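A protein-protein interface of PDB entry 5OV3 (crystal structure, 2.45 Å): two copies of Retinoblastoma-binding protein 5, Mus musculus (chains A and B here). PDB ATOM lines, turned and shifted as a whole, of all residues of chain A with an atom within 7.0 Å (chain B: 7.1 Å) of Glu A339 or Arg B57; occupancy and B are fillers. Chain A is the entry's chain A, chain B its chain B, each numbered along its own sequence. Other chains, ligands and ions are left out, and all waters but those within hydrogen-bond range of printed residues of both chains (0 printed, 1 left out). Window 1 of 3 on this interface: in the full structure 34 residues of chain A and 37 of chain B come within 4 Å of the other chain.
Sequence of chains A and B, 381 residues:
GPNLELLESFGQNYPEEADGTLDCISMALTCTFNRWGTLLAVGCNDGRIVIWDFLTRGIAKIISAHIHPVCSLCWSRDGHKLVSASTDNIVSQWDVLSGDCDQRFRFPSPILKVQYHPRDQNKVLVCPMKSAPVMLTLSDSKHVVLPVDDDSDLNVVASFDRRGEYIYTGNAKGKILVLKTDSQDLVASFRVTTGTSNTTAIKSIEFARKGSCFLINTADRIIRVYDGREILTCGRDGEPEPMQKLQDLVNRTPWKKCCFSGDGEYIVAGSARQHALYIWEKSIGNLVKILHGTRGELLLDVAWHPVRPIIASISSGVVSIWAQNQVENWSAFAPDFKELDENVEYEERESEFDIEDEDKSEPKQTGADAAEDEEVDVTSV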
ATOM      1  N   ASP A  53      35.576  20.957  18.132  1.00  0.00           N
ATOM      2  CA  ASP A  53      35.699  22.390  18.381  1.00  0.00           C
ATOM      3  C   ASP A  53      34.319  22.969  18.686  1.00  0.00           C
ATOM      4  O   ASP A  53      33.394  22.857  17.876  1.00  0.00           O
ATOM      5  CB  ASP A  53      36.350  23.067  17.168  1.00  0.00           C
ATOM      6  CG  ASP A  53      36.484  24.588  17.309  1.00  0.00           C
ATOM      7  OD1 ASP A  53      36.777  25.116  18.404  1.00  0.00           O
ATOM      8  OD2 ASP A  53      36.305  25.271  16.282  1.00  0.00           O
ATOM      9  N   PHE A  54      34.176  23.557  19.869  1.00  0.00           N
ATOM     10  CA  PHE A  54      32.929  24.211  20.232  1.00  0.00           C
ATOM     11  C   PHE A  54      32.680  25.497  19.438  1.00  0.00           C
ATOM     12  O   PHE A  54      31.531  25.932  19.338  1.00  0.00           O
ATOM     13  CB  PHE A  54      32.925  24.516  21.726  1.00  0.00           C
ATOM     14  CG  PHE A  54      32.314  23.417  22.568  1.00  0.00           C
ATOM     15  CD1 PHE A  54      32.984  22.231  22.770  1.00  0.00           C
ATOM     16  CD2 PHE A  54      31.077  23.587  23.161  1.00  0.00           C
ATOM     17  CE1 PHE A  54      32.421  21.225  23.530  1.00  0.00           C
ATOM     18  CE2 PHE A  54      30.508  22.594  23.922  1.00  0.00           C
ATOM     19  CZ  PHE A  54      31.180  21.404  24.110  1.00  0.00           C
ATOM     20  N   LEU A  55      33.715  26.113  18.869  1.00  0.00           N
ATOM     21  CA  LEU A  55      33.495  27.371  18.161  1.00  0.00           C
ATOM     22  C   LEU A  55      32.972  27.129  16.749  1.00  0.00           C
ATOM     23  O   LEU A  55      31.906  27.633  16.390  1.00  0.00           O
ATOM     24  CB  LEU A  55      34.776  28.203  18.147  1.00  0.00           C
ATOM     25  CG  LEU A  55      35.284  28.520  19.556  1.00  0.00           C
ATOM     26  CD1 LEU A  55      36.493  29.415  19.520  1.00  0.00           C
ATOM     27  CD2 LEU A  55      34.196  29.153  20.366  1.00  0.00           C
ATOM     28  N   THR A  56      33.676  26.314  15.955  1.00  0.00           N
ATOM     29  CA  THR A  56      33.184  25.974  14.622  1.00  0.00           C
ATOM     30  C   THR A  56      32.131  24.877  14.623  1.00  0.00           C
ATOM     31  O   THR A  56      31.591  24.577  13.553  1.00  0.00           O
ATOM     32  CB  THR A  56      34.306  25.493  13.703  1.00  0.00           C
ATOM     33  OG1 THR A  56      34.839  24.258  14.215  1.00  0.00           O
ATOM     34  CG2 THR A  56      35.398  26.543  13.582  1.00  0.00           C
ATOM     35  N   ARG A  57      31.863  24.249  15.767  1.00  0.00           N
ATOM     36  CA  ARG A  57      31.014  23.058  15.823  1.00  0.00           C
ATOM     37  C   ARG A  57      31.469  22.010  14.800  1.00  0.00           C
ATOM     38  O   ARG A  57      30.671  21.389  14.101  1.00  0.00           O
ATOM     39  CB  ARG A  57      29.546  23.441  15.643  1.00  0.00           C
ATOM     40  CG  ARG A  57      29.111  24.499  16.656  1.00  0.00           C
ATOM     41  CD  ARG A  57      27.721  24.277  17.218  1.00  0.00           C
ATOM     42  NE  ARG A  57      26.697  24.902  16.388  1.00  0.00           N
ATOM     43  CZ  ARG A  57      25.892  24.240  15.562  1.00  0.00           C
ATOM     44  NH1 ARG A  57      25.987  22.916  15.467  1.00  0.00           N
ATOM     45  NH2 ARG A  57      24.994  24.903  14.832  1.00  0.00           N
ATOM     46  N   ILE A 310      27.268  23.314  30.636  1.00  0.00           N
ATOM     47  CA  ILE A 310      27.262  22.336  29.565  1.00  0.00           C
ATOM     48  C   ILE A 310      27.827  21.044  30.138  1.00  0.00           C
ATOM     49  O   ILE A 310      28.757  21.082  30.952  1.00  0.00           O
ATOM     50  CB  ILE A 310      28.110  22.818  28.366  1.00  0.00           C
ATOM     51  CG1 ILE A 310      27.501  24.065  27.728  1.00  0.00           C
ATOM     52  CG2 ILE A 310      28.329  21.704  27.349  1.00  0.00           C
ATOM     53  CD1 ILE A 310      28.468  24.781  26.785  1.00  0.00           C
ATOM     54  N   ALA A 323      23.031  21.397  27.133  1.00  0.00           N
ATOM     55  CA  ALA A 323      23.362  22.778  27.432  1.00  0.00           C
ATOM     56  C   ALA A 323      22.148  23.499  27.982  1.00  0.00           C
ATOM     57  O   ALA A 323      21.011  23.041  27.878  1.00  0.00           O
ATOM     58  CB  ALA A 323      23.910  23.511  26.207  1.00  0.00           C
ATOM     59  N   ASN A 325      20.784  27.521  28.206  1.00  0.00           N
ATOM     60  CA  ASN A 325      20.895  28.942  27.918  1.00  0.00           C
ATOM     61  C   ASN A 325      20.130  29.729  28.969  1.00  0.00           C
ATOM     62  O   ASN A 325      19.256  29.194  29.657  1.00  0.00           O
ATOM     63  CB  ASN A 325      20.360  29.271  26.526  1.00  0.00           C
ATOM     64  CG  ASN A 325      20.904  28.353  25.455  1.00  0.00           C
ATOM     65  OD1 ASN A 325      22.024  28.538  24.971  1.00  0.00           O
ATOM     66  ND2 ASN A 325      20.108  27.359  25.067  1.00  0.00           N
ATOM     67  N   ASN A 329      16.699  34.286  25.275  1.00  0.00           N
ATOM     68  CA  ASN A 329      16.734  33.548  24.018  1.00  0.00           C
ATOM     69  C   ASN A 329      15.446  33.635  23.205  1.00  0.00           C
ATOM     70  O   ASN A 329      15.455  33.292  22.016  1.00  0.00           O
ATOM     71  CB  ASN A 329      17.140  32.100  24.264  1.00  0.00           C
ATOM     72  CG  ASN A 329      18.610  31.881  23.972  1.00  0.00           C
ATOM     73  OD1 ASN A 329      19.390  31.536  24.857  1.00  0.00           O
ATOM     74  ND2 ASN A 329      19.005  32.135  22.726  1.00  0.00           N
ATOM     75  N   PHE A 337      19.445  35.549  15.220  1.00  0.00           N
ATOM     76  CA  PHE A 337      20.759  34.990  14.936  1.00  0.00           C
ATOM     77  C   PHE A 337      20.561  33.803  14.014  1.00  0.00           C
ATOM     78  O   PHE A 337      19.793  32.892  14.326  1.00  0.00           O
ATOM     79  CB  PHE A 337      21.470  34.533  16.220  1.00  0.00           C
ATOM     80  CG  PHE A 337      21.982  35.661  17.060  1.00  0.00           C
ATOM     81  CD1 PHE A 337      21.123  36.364  17.906  1.00  0.00           C
ATOM     82  CD2 PHE A 337      23.328  36.032  17.007  1.00  0.00           C
ATOM     83  CE1 PHE A 337      21.589  37.443  18.687  1.00  0.00           C
ATOM     84  CE2 PHE A 337      23.810  37.098  17.775  1.00  0.00           C
ATOM     85  CZ  PHE A 337      22.927  37.811  18.619  1.00  0.00           C
ATOM     86  N   LYS A 338      21.227  33.804  12.882  1.00  0.00           N
ATOM     87  CA  LYS A 338      21.166  32.644  12.024  1.00  0.00           C
ATOM     88  C   LYS A 338      22.588  32.207  11.727  1.00  0.00           C
ATOM     89  O   LYS A 338      23.507  33.029  11.670  1.00  0.00           O
ATOM     90  CB  LYS A 338      20.342  32.912  10.736  1.00  0.00           C
ATOM     91  CG  LYS A 338      20.845  33.977   9.767  1.00  0.00           C
ATOM     92  CD  LYS A 338      20.031  33.914   8.453  1.00  0.00           C
ATOM     93  CE  LYS A 338      20.605  34.809   7.350  1.00  0.00           C
ATOM     94  NZ  LYS A 338      20.176  34.411   5.962  1.00  0.00           N
ATOM     95  N   GLU A 339      22.772  30.907  11.586  1.00  0.00           N
ATOM     96  CA  GLU A 339      24.086  30.318  11.431  1.00  0.00           C
ATOM     97  C   GLU A 339      24.142  29.633  10.090  1.00  0.00           C
ATOM     98  O   GLU A 339      23.250  28.857   9.753  1.00  0.00           O
ATOM     99  CB  GLU A 339      24.380  29.310  12.545  1.00  0.00           C
ATOM    100  CG  GLU A 339      25.676  28.547  12.333  1.00  0.00           C
ATOM    101  CD  GLU A 339      26.359  28.184  13.631  1.00  0.00           C
ATOM    102  OE1 GLU A 339      27.420  27.524  13.563  1.00  0.00           O
ATOM    103  OE2 GLU A 339      25.844  28.559  14.713  1.00  0.00           O
ATOM    104  N   LEU A 340      25.186  29.910   9.332  1.00  0.00           N
ATOM    105  CA  LEU A 340      25.396  29.275   8.046  1.00  0.00           C
ATOM    106  C   LEU A 340      26.683  28.487   8.178  1.00  0.00           C
ATOM    107  O   LEU A 340      27.742  29.070   8.417  1.00  0.00           O
ATOM    108  CB  LEU A 340      25.464  30.329   6.937  1.00  0.00           C
ATOM    109  CG  LEU A 340      24.303  31.253   7.095  1.00  0.00           C
ATOM    110  CD1 LEU A 340      24.584  32.568   6.662  1.00  0.00           C
ATOM    111  CD2 LEU A 340      23.109  30.764   6.410  1.00  0.00           C
ATOM    112  N   ASP A 341      26.577  27.169   8.099  1.00  0.00           N
ATOM    113  CA  ASP A 341      27.692  26.265   8.345  1.00  0.00           C
ATOM    114  C   ASP A 341      28.139  25.664   7.025  1.00  0.00           C
ATOM    115  O   ASP A 341      27.311  25.182   6.247  1.00  0.00           O
ATOM    116  CB  ASP A 341      27.292  25.147   9.319  1.00  0.00           C
ATOM    117  CG  ASP A 341      27.146  25.644  10.752  1.00  0.00           C
ATOM    118  OD1 ASP A 341      28.135  26.172  11.317  1.00  0.00           O
ATOM    119  OD2 ASP A 341      26.029  25.532  11.303  1.00  0.00           O
ATOM    120  N   TRP B  52      26.343  37.354  22.888  1.00  0.00           N
ATOM    121  CA  TRP B  52      25.995  36.054  22.338  1.00  0.00           C
ATOM    122  C   TRP B  52      27.187  35.122  22.532  1.00  0.00           C
ATOM    123  O   TRP B  52      28.336  35.504  22.268  1.00  0.00           O
ATOM    124  CB  TRP B  52      25.588  36.175  20.861  1.00  0.00           C
ATOM    125  CG  TRP B  52      24.931  34.948  20.293  1.00  0.00           C
ATOM    126  CD1 TRP B  52      23.603  34.610  20.362  1.00  0.00           C
ATOM    127  CD2 TRP B  52      25.568  33.901  19.553  1.00  0.00           C
ATOM    128  NE1 TRP B  52      23.389  33.418  19.717  1.00  0.00           N
ATOM    129  CE2 TRP B  52      24.577  32.962  19.214  1.00  0.00           C
ATOM    130  CE3 TRP B  52      26.887  33.665  19.152  1.00  0.00           C
ATOM    131  CZ2 TRP B  52      24.860  31.810  18.491  1.00  0.00           C
ATOM    132  CZ3 TRP B  52      27.171  32.514  18.430  1.00  0.00           C
ATOM    133  CH2 TRP B  52      26.161  31.603  18.106  1.00  0.00           C
ATOM    134  N   ASP B  53      26.899  33.911  23.003  1.00  0.00           N
ATOM    135  CA  ASP B  53      27.883  32.957  23.499  1.00  0.00           C
ATOM    136  C   ASP B  53      28.087  31.856  22.470  1.00  0.00           C
ATOM    137  O   ASP B  53      27.154  31.093  22.192  1.00  0.00           O
ATOM    138  CB  ASP B  53      27.389  32.360  24.823  1.00  0.00           C
ATOM    139  CG  ASP B  53      28.325  31.308  25.402  1.00  0.00           C
ATOM    140  OD1 ASP B  53      29.547  31.317  25.125  1.00  0.00           O
ATOM    141  OD2 ASP B  53      27.838  30.473  26.179  1.00  0.00           O
ATOM    142  N   PHE B  54      29.307  31.746  21.936  1.00  0.00           N
ATOM    143  CA  PHE B  54      29.580  30.659  21.001  1.00  0.00           C
ATOM    144  C   PHE B  54      29.535  29.287  21.664  1.00  0.00           C
ATOM    145  O   PHE B  54      29.195  28.297  21.003  1.00  0.00           O
ATOM    146  CB  PHE B  54      30.923  30.868  20.323  1.00  0.00           C
ATOM    147  CG  PHE B  54      30.833  31.734  19.095  1.00  0.00           C
ATOM    148  CD1 PHE B  54      30.734  33.117  19.213  1.00  0.00           C
ATOM    149  CD2 PHE B  54      30.798  31.159  17.830  1.00  0.00           C
ATOM    150  CE1 PHE B  54      30.624  33.919  18.100  1.00  0.00           C
ATOM    151  CE2 PHE B  54      30.696  31.941  16.706  1.00  0.00           C
ATOM    152  CZ  PHE B  54      30.608  33.339  16.831  1.00  0.00           C
ATOM    153  N   LEU B  55      29.863  29.184  22.951  1.00  0.00           N
ATOM    154  CA  LEU B  55      29.913  27.856  23.552  1.00  0.00           C
ATOM    155  C   LEU B  55      28.517  27.261  23.676  1.00  0.00           C
ATOM    156  O   LEU B  55      28.289  26.126  23.256  1.00  0.00           O
ATOM    157  CB  LEU B  55      30.625  27.901  24.904  1.00  0.00           C
ATOM    158  CG  LEU B  55      32.027  28.502  24.793  1.00  0.00           C
ATOM    159  CD1 LEU B  55      32.647  28.670  26.145  1.00  0.00           C
ATOM    160  CD2 LEU B  55      32.922  27.701  23.864  1.00  0.00           C
ATOM    161  N   THR B  56      27.558  28.023  24.214  1.00  0.00           N
ATOM    162  CA  THR B  56      26.181  27.547  24.322  1.00  0.00           C
ATOM    163  C   THR B  56      25.314  27.852  23.100  1.00  0.00           C
ATOM    164  O   THR B  56      24.185  27.346  23.042  1.00  0.00           O
ATOM    165  CB  THR B  56      25.462  28.144  25.551  1.00  0.00           C
ATOM    166  OG1 THR B  56      25.300  29.561  25.393  1.00  0.00           O
ATOM    167  CG2 THR B  56      26.194  27.842  26.840  1.00  0.00           C
ATOM    168  N   ARG B  57      25.775  28.680  22.150  1.00  0.00           N
ATOM    169  CA  ARG B  57      24.987  29.017  20.954  1.00  0.00           C
ATOM    170  C   ARG B  57      23.654  29.676  21.331  1.00  0.00           C
ATOM    171  O   ARG B  57      22.590  29.334  20.813  1.00  0.00           O
ATOM    172  CB  ARG B  57      24.756  27.777  20.084  1.00  0.00           C
ATOM    173  CG  ARG B  57      25.308  27.875  18.672  1.00  0.00           C
ATOM    174  CD  ARG B  57      26.816  27.974  18.700  1.00  0.00           C
ATOM    175  NE  ARG B  57      27.417  27.948  17.368  1.00  0.00           N
ATOM    176  CZ  ARG B  57      28.729  27.915  17.140  1.00  0.00           C
ATOM    177  NH1 ARG B  57      29.180  27.889  15.895  1.00  0.00           N
ATOM    178  NH2 ARG B  57      29.595  27.907  18.152  1.00  0.00           N
ATOM    179  N   GLY B  58      23.721  30.632  22.250  1.00  0.00           N
ATOM    180  CA  GLY B  58      22.542  31.355  22.684  1.00  0.00           C
ATOM    181  C   GLY B  58      22.982  32.595  23.426  1.00  0.00           C
ATOM    182  O   GLY B  58      24.174  32.855  23.580  1.00  0.00           O
ATOM    183  N   ILE B  59      22.009  33.362  23.896  1.00  0.00           N
ATOM    184  CA  ILE B  59      22.310  34.648  24.514  1.00  0.00           C
ATOM    185  C   ILE B  59      22.745  34.441  25.955  1.00  0.00           C
ATOM    186  O   ILE B  59      22.054  33.776  26.736  1.00  0.00           O
ATOM    187  CB  ILE B  59      21.101  35.588  24.420  1.00  0.00           C
ATOM    188  CG1 ILE B  59      20.962  36.085  22.983  1.00  0.00           C
ATOM    189  CG2 ILE B  59      21.246  36.763  25.381  1.00  0.00           C
ATOM    190  CD1 ILE B  59      19.566  36.305  22.606  1.00  0.00           C
ATOM    191  N   ILE B 310      35.571  31.781  11.076  1.00  0.00           N
ATOM    192  CA  ILE B 310      34.201  32.203  11.329  1.00  0.00           C
ATOM    193  C   ILE B 310      34.072  33.690  11.023  1.00  0.00           C
ATOM    194  O   ILE B 310      34.924  34.501  11.414  1.00  0.00           O
ATOM    195  CB  ILE B 310      33.780  31.903  12.783  1.00  0.00           C
ATOM    196  CG1 ILE B 310      33.695  30.390  13.017  1.00  0.00           C
ATOM    197  CG2 ILE B 310      32.450  32.572  13.112  1.00  0.00           C
ATOM    198  CD1 ILE B 310      33.761  30.035  14.472  1.00  0.00           C
ATOM    199  N   VAL B 319      21.775  38.897  12.658  1.00  0.00           N
ATOM    200  CA  VAL B 319      23.160  38.437  12.792  1.00  0.00           C
ATOM    201  C   VAL B 319      23.337  37.115  12.051  1.00  0.00           C
ATOM    202  O   VAL B 319      22.534  36.189  12.218  1.00  0.00           O
ATOM    203  CB  VAL B 319      23.543  38.270  14.273  1.00  0.00           C
ATOM    204  CG1 VAL B 319      25.022  37.937  14.398  1.00  0.00           C
ATOM    205  CG2 VAL B 319      23.217  39.516  15.054  1.00  0.00           C
ATOM    206  N   SER B 320      24.391  37.017  11.237  1.00  0.00           N
ATOM    207  CA  SER B 320      24.736  35.783  10.535  1.00  0.00           C
ATOM    208  C   SER B 320      26.110  35.337  10.978  1.00  0.00           C
ATOM    209  O   SER B 320      27.058  36.127  10.939  1.00  0.00           O
ATOM    210  CB  SER B 320      24.758  35.935   9.011  1.00  0.00           C
ATOM    211  OG  SER B 320      23.466  36.170   8.495  1.00  0.00           O
ATOM    212  N   ILE B 321      26.213  34.079  11.385  1.00  0.00           N
ATOM    213  CA  ILE B 321      27.485  33.437  11.682  1.00  0.00           C
ATOM    214  C   ILE B 321      27.785  32.500  10.525  1.00  0.00           C
ATOM    215  O   ILE B 321      27.037  31.545  10.276  1.00  0.00           O
ATOM    216  CB  ILE B 321      27.447  32.684  13.015  1.00  0.00           C
ATOM    217  CG1 ILE B 321      26.882  33.596  14.105  1.00  0.00           C
ATOM    218  CG2 ILE B 321      28.837  32.213  13.379  1.00  0.00           C
ATOM    219  CD1 ILE B 321      27.716  34.868  14.321  1.00  0.00           C
ATOM    220  N   TRP B 322      28.846  32.800   9.781  1.00  0.00           N
ATOM    221  CA  TRP B 322      29.319  31.931   8.718  1.00  0.00           C
ATOM    222  C   TRP B 322      30.502  31.164   9.276  1.00  0.00           C
ATOM    223  O   TRP B 322      31.493  31.776   9.703  1.00  0.00           O
ATOM    224  CB  TRP B 322      29.753  32.704   7.479  1.00  0.00           C
ATOM    225  CG  TRP B 322      28.818  33.786   7.015  1.00  0.00           C
ATOM    226  CD1 TRP B 322      28.606  35.009   7.608  1.00  0.00           C
ATOM    227  CD2 TRP B 322      28.007  33.771   5.829  1.00  0.00           C
ATOM    228  NE1 TRP B 322      27.701  35.732   6.875  1.00  0.00           N
ATOM    229  CE2 TRP B 322      27.324  35.006   5.776  1.00  0.00           C
ATOM    230  CE3 TRP B 322      27.796  32.833   4.807  1.00  0.00           C
ATOM    231  CZ2 TRP B 322      26.451  35.332   4.741  1.00  0.00           C
ATOM    232  CZ3 TRP B 322      26.917  33.156   3.783  1.00  0.00           C
ATOM    233  CH2 TRP B 322      26.259  34.395   3.759  1.00  0.00           C
ATOM    234  N   ALA B 323      30.390  29.836   9.295  1.00  0.00           N
ATOM    235  CA  ALA B 323      31.419  28.994   9.878  1.00  0.00           C
ATOM    236  C   ALA B 323      31.762  27.850   8.937  1.00  0.00           C
ATOM    237  O   ALA B 323      30.872  27.218   8.357  1.00  0.00           O
ATOM    238  CB  ALA B 323      30.973  28.434  11.230  1.00  0.00           C
ATOM    239  N   ASN B 325      33.078  24.118   9.085  1.00  0.00           N
ATOM    240  CA  ASN B 325      33.113  23.014  10.044  1.00  0.00           C
ATOM    241  C   ASN B 325      33.807  21.828   9.389  1.00  0.00           C
ATOM    242  O   ASN B 325      33.301  21.275   8.407  1.00  0.00           O
ATOM    243  CB  ASN B 325      31.706  22.626  10.497  1.00  0.00           C
ATOM    244  CG  ASN B 325      30.685  23.679  10.174  1.00  0.00           C
ATOM    245  OD1 ASN B 325      29.964  23.569   9.196  1.00  0.00           O
ATOM    246  ND2 ASN B 325      30.618  24.717  10.998  1.00  0.00           N
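O of Phe A54 sits at hydrogen-bond distance from NH2 of Arg B57 (3.0 Å).
The backbone carbonyl oxygen (O) of Leu A55 lies within hydrogen-bond range of the guanidinium group (NH1) of Arg B57.
The side-chain amide nitrogen (ND2) of Asn B325 is in hydrogen-bond range of the backbone carbonyl oxygen (O) of Thr A56 (2.7 Å).
The backbone carbonyl oxygen (O) of Thr B56 sits close to the side-chain amide oxygen (OD1) of Asn A325 (3.1 Å).
The side-chain amide oxygen of Asn A329 lies within hydrogen-bond range of the backbone NH of Ile B59 (3.3 Å).
The backbone NH (N) of Lys A338 sits at hydrogen-bond distance from the backbone carbonyl oxygen (O) of Val B319 (2.8 Å).
The backbone NH of Ile B321 is in hydrogen-bond range of the backbone carbonyl oxygen of Lys A338.
NH1 of Arg B57 lies within salt-bridge range of OE1 of Glu A339, 2.9 Å away.
The backbone NH (N) of Leu A340 lies within hydrogen-bond range of the backbone carbonyl oxygen (O) of Ile B321 (2.6 Å).
The backbone carbonyl oxygen (O) of Leu A340 sits at hydrogen-bond distance from the backbone NH (N) of Ala B323 (2.9 Å).
The side-chain amide nitrogen of Asn B325 sits at hydrogen-bond distance from the side-chain carboxylate of Asp A341 (2.9 Å).
The guanidinium group (NE) of Arg B57 sits close to the guanidinium group (NE) of Arg A57, at 3.3 Å.
OD1 of Asp A53 sits close to N of Leu A55 (3.3 Å).
The side-chain carboxylate (OD2) of Asp A53 sits at hydrogen-bond distance from the side-chain hydroxyl (OG1) of Thr A56, 2.7 Å away.
The side-chain carboxylate of Glu A339 is in salt-bridge range of the guanidinium group of Arg A57 (3.8 Å).
The guanidinium group (NH2) of Arg A57 lies within salt-bridge range of the side-chain carboxylate (OD2) of Asp A341.
The side-chain carboxylate (OE1) of Glu A339 lies close to the side-chain carboxylate (OD1) of Asp A341, at 2.7 Å.
OD2 of Asp B53 is in hydrogen-bond range of OG1 of Thr B56.
Phe A54 touches Phe B54 (O to O, 3.7 Å).
Leu A55 touches Leu B55 (CD2 to CD2, 3.996 Å).
CD1 of Ile B310 touches CG2 of Thr A56, 3.96 Å away.
O of Arg A57 touches CB of Asn B325, 3.9 Å away.
Ile A310 touches Leu B55 (CD1 to O, 3.8 Å).
OD1 of Asn A325 touches CA of Gly B58, at 3.7 Å.
ND2 of Asn A329 touches CA of Gly B58, at 3.6 Å.
Phe A337 touches Trp B52 (CE2 to CG, 3.5 Å).
Phe A337 touches Val B319.
CA of Glu A339 touches O of Ile B321, at 3.4 Å.
Of the printed residues of chain A, Leu B55 touches Phe A54 (3.8 Å), Leu A55 (3.996 Å) and Ile A310 (3.8 Å).
Of chain A, only Phe A54, Leu A55, Arg A57 and Glu A339 come within 4 Å of Arg B57.
Printed residues of chain A within 4 Å of Ile B59: Asn A329 (3.3 Å).
Printed residues of chain A within 4 Å of Ser B320: Lys A338 (3.2 Å).
Of the printed residues of chain A, Ala B323 touches Leu A340 (2.9 Å) and Asp A341 (3.3 Å).
The nearest residue of chain B that does not touch Glu A339 is Ala B323 (4.3 Å).
Of the 14 printed residues of chain A, 12 touch a printed residue of chain B.
Hydrophobic or aromatic side chains of chain A that line the printed part of chain B: Phe A54, Leu A55, Ile A310, Phe A337 and Leu A340.
Along chain A the printed residues that touch a printed residue of chain B span positions 54 to 341.
Hydrophobic or aromatic side chains of chain B that line the printed part of chain A: Trp B52, Phe B54, Leu B55, Ile B310, Val B319, Trp B322 and Ala B323.
Along chain B the printed residues that touch a printed residue of chain A span positions 52 to 325.
Among the printed residues, 29 pairs touch across the chains.
Among the printed residues, Asp or Glu carboxylates within 4 Å of a Lys or Arg side-chain nitrogen of the other chain: Glu A339 with Arg B57.
Phe A54 touches Leu B55, and with the chains exchanged Leu A55 touches Phe B54.
Phe A54 touches Arg B57, but with the chains exchanged Arg A57 does not touch Phe B54 (5.7 Å).
Leu A55 touches its own counterpart, Leu B55.
Thr A56 touches Ile B310, and with the chains exchanged Ile A310 touches Thr B56.
8 positions are printed for both chains.
Of the 29 pairs that touch across the chains among the printed residues, 11 have their exchanged pair printed and touching as well.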
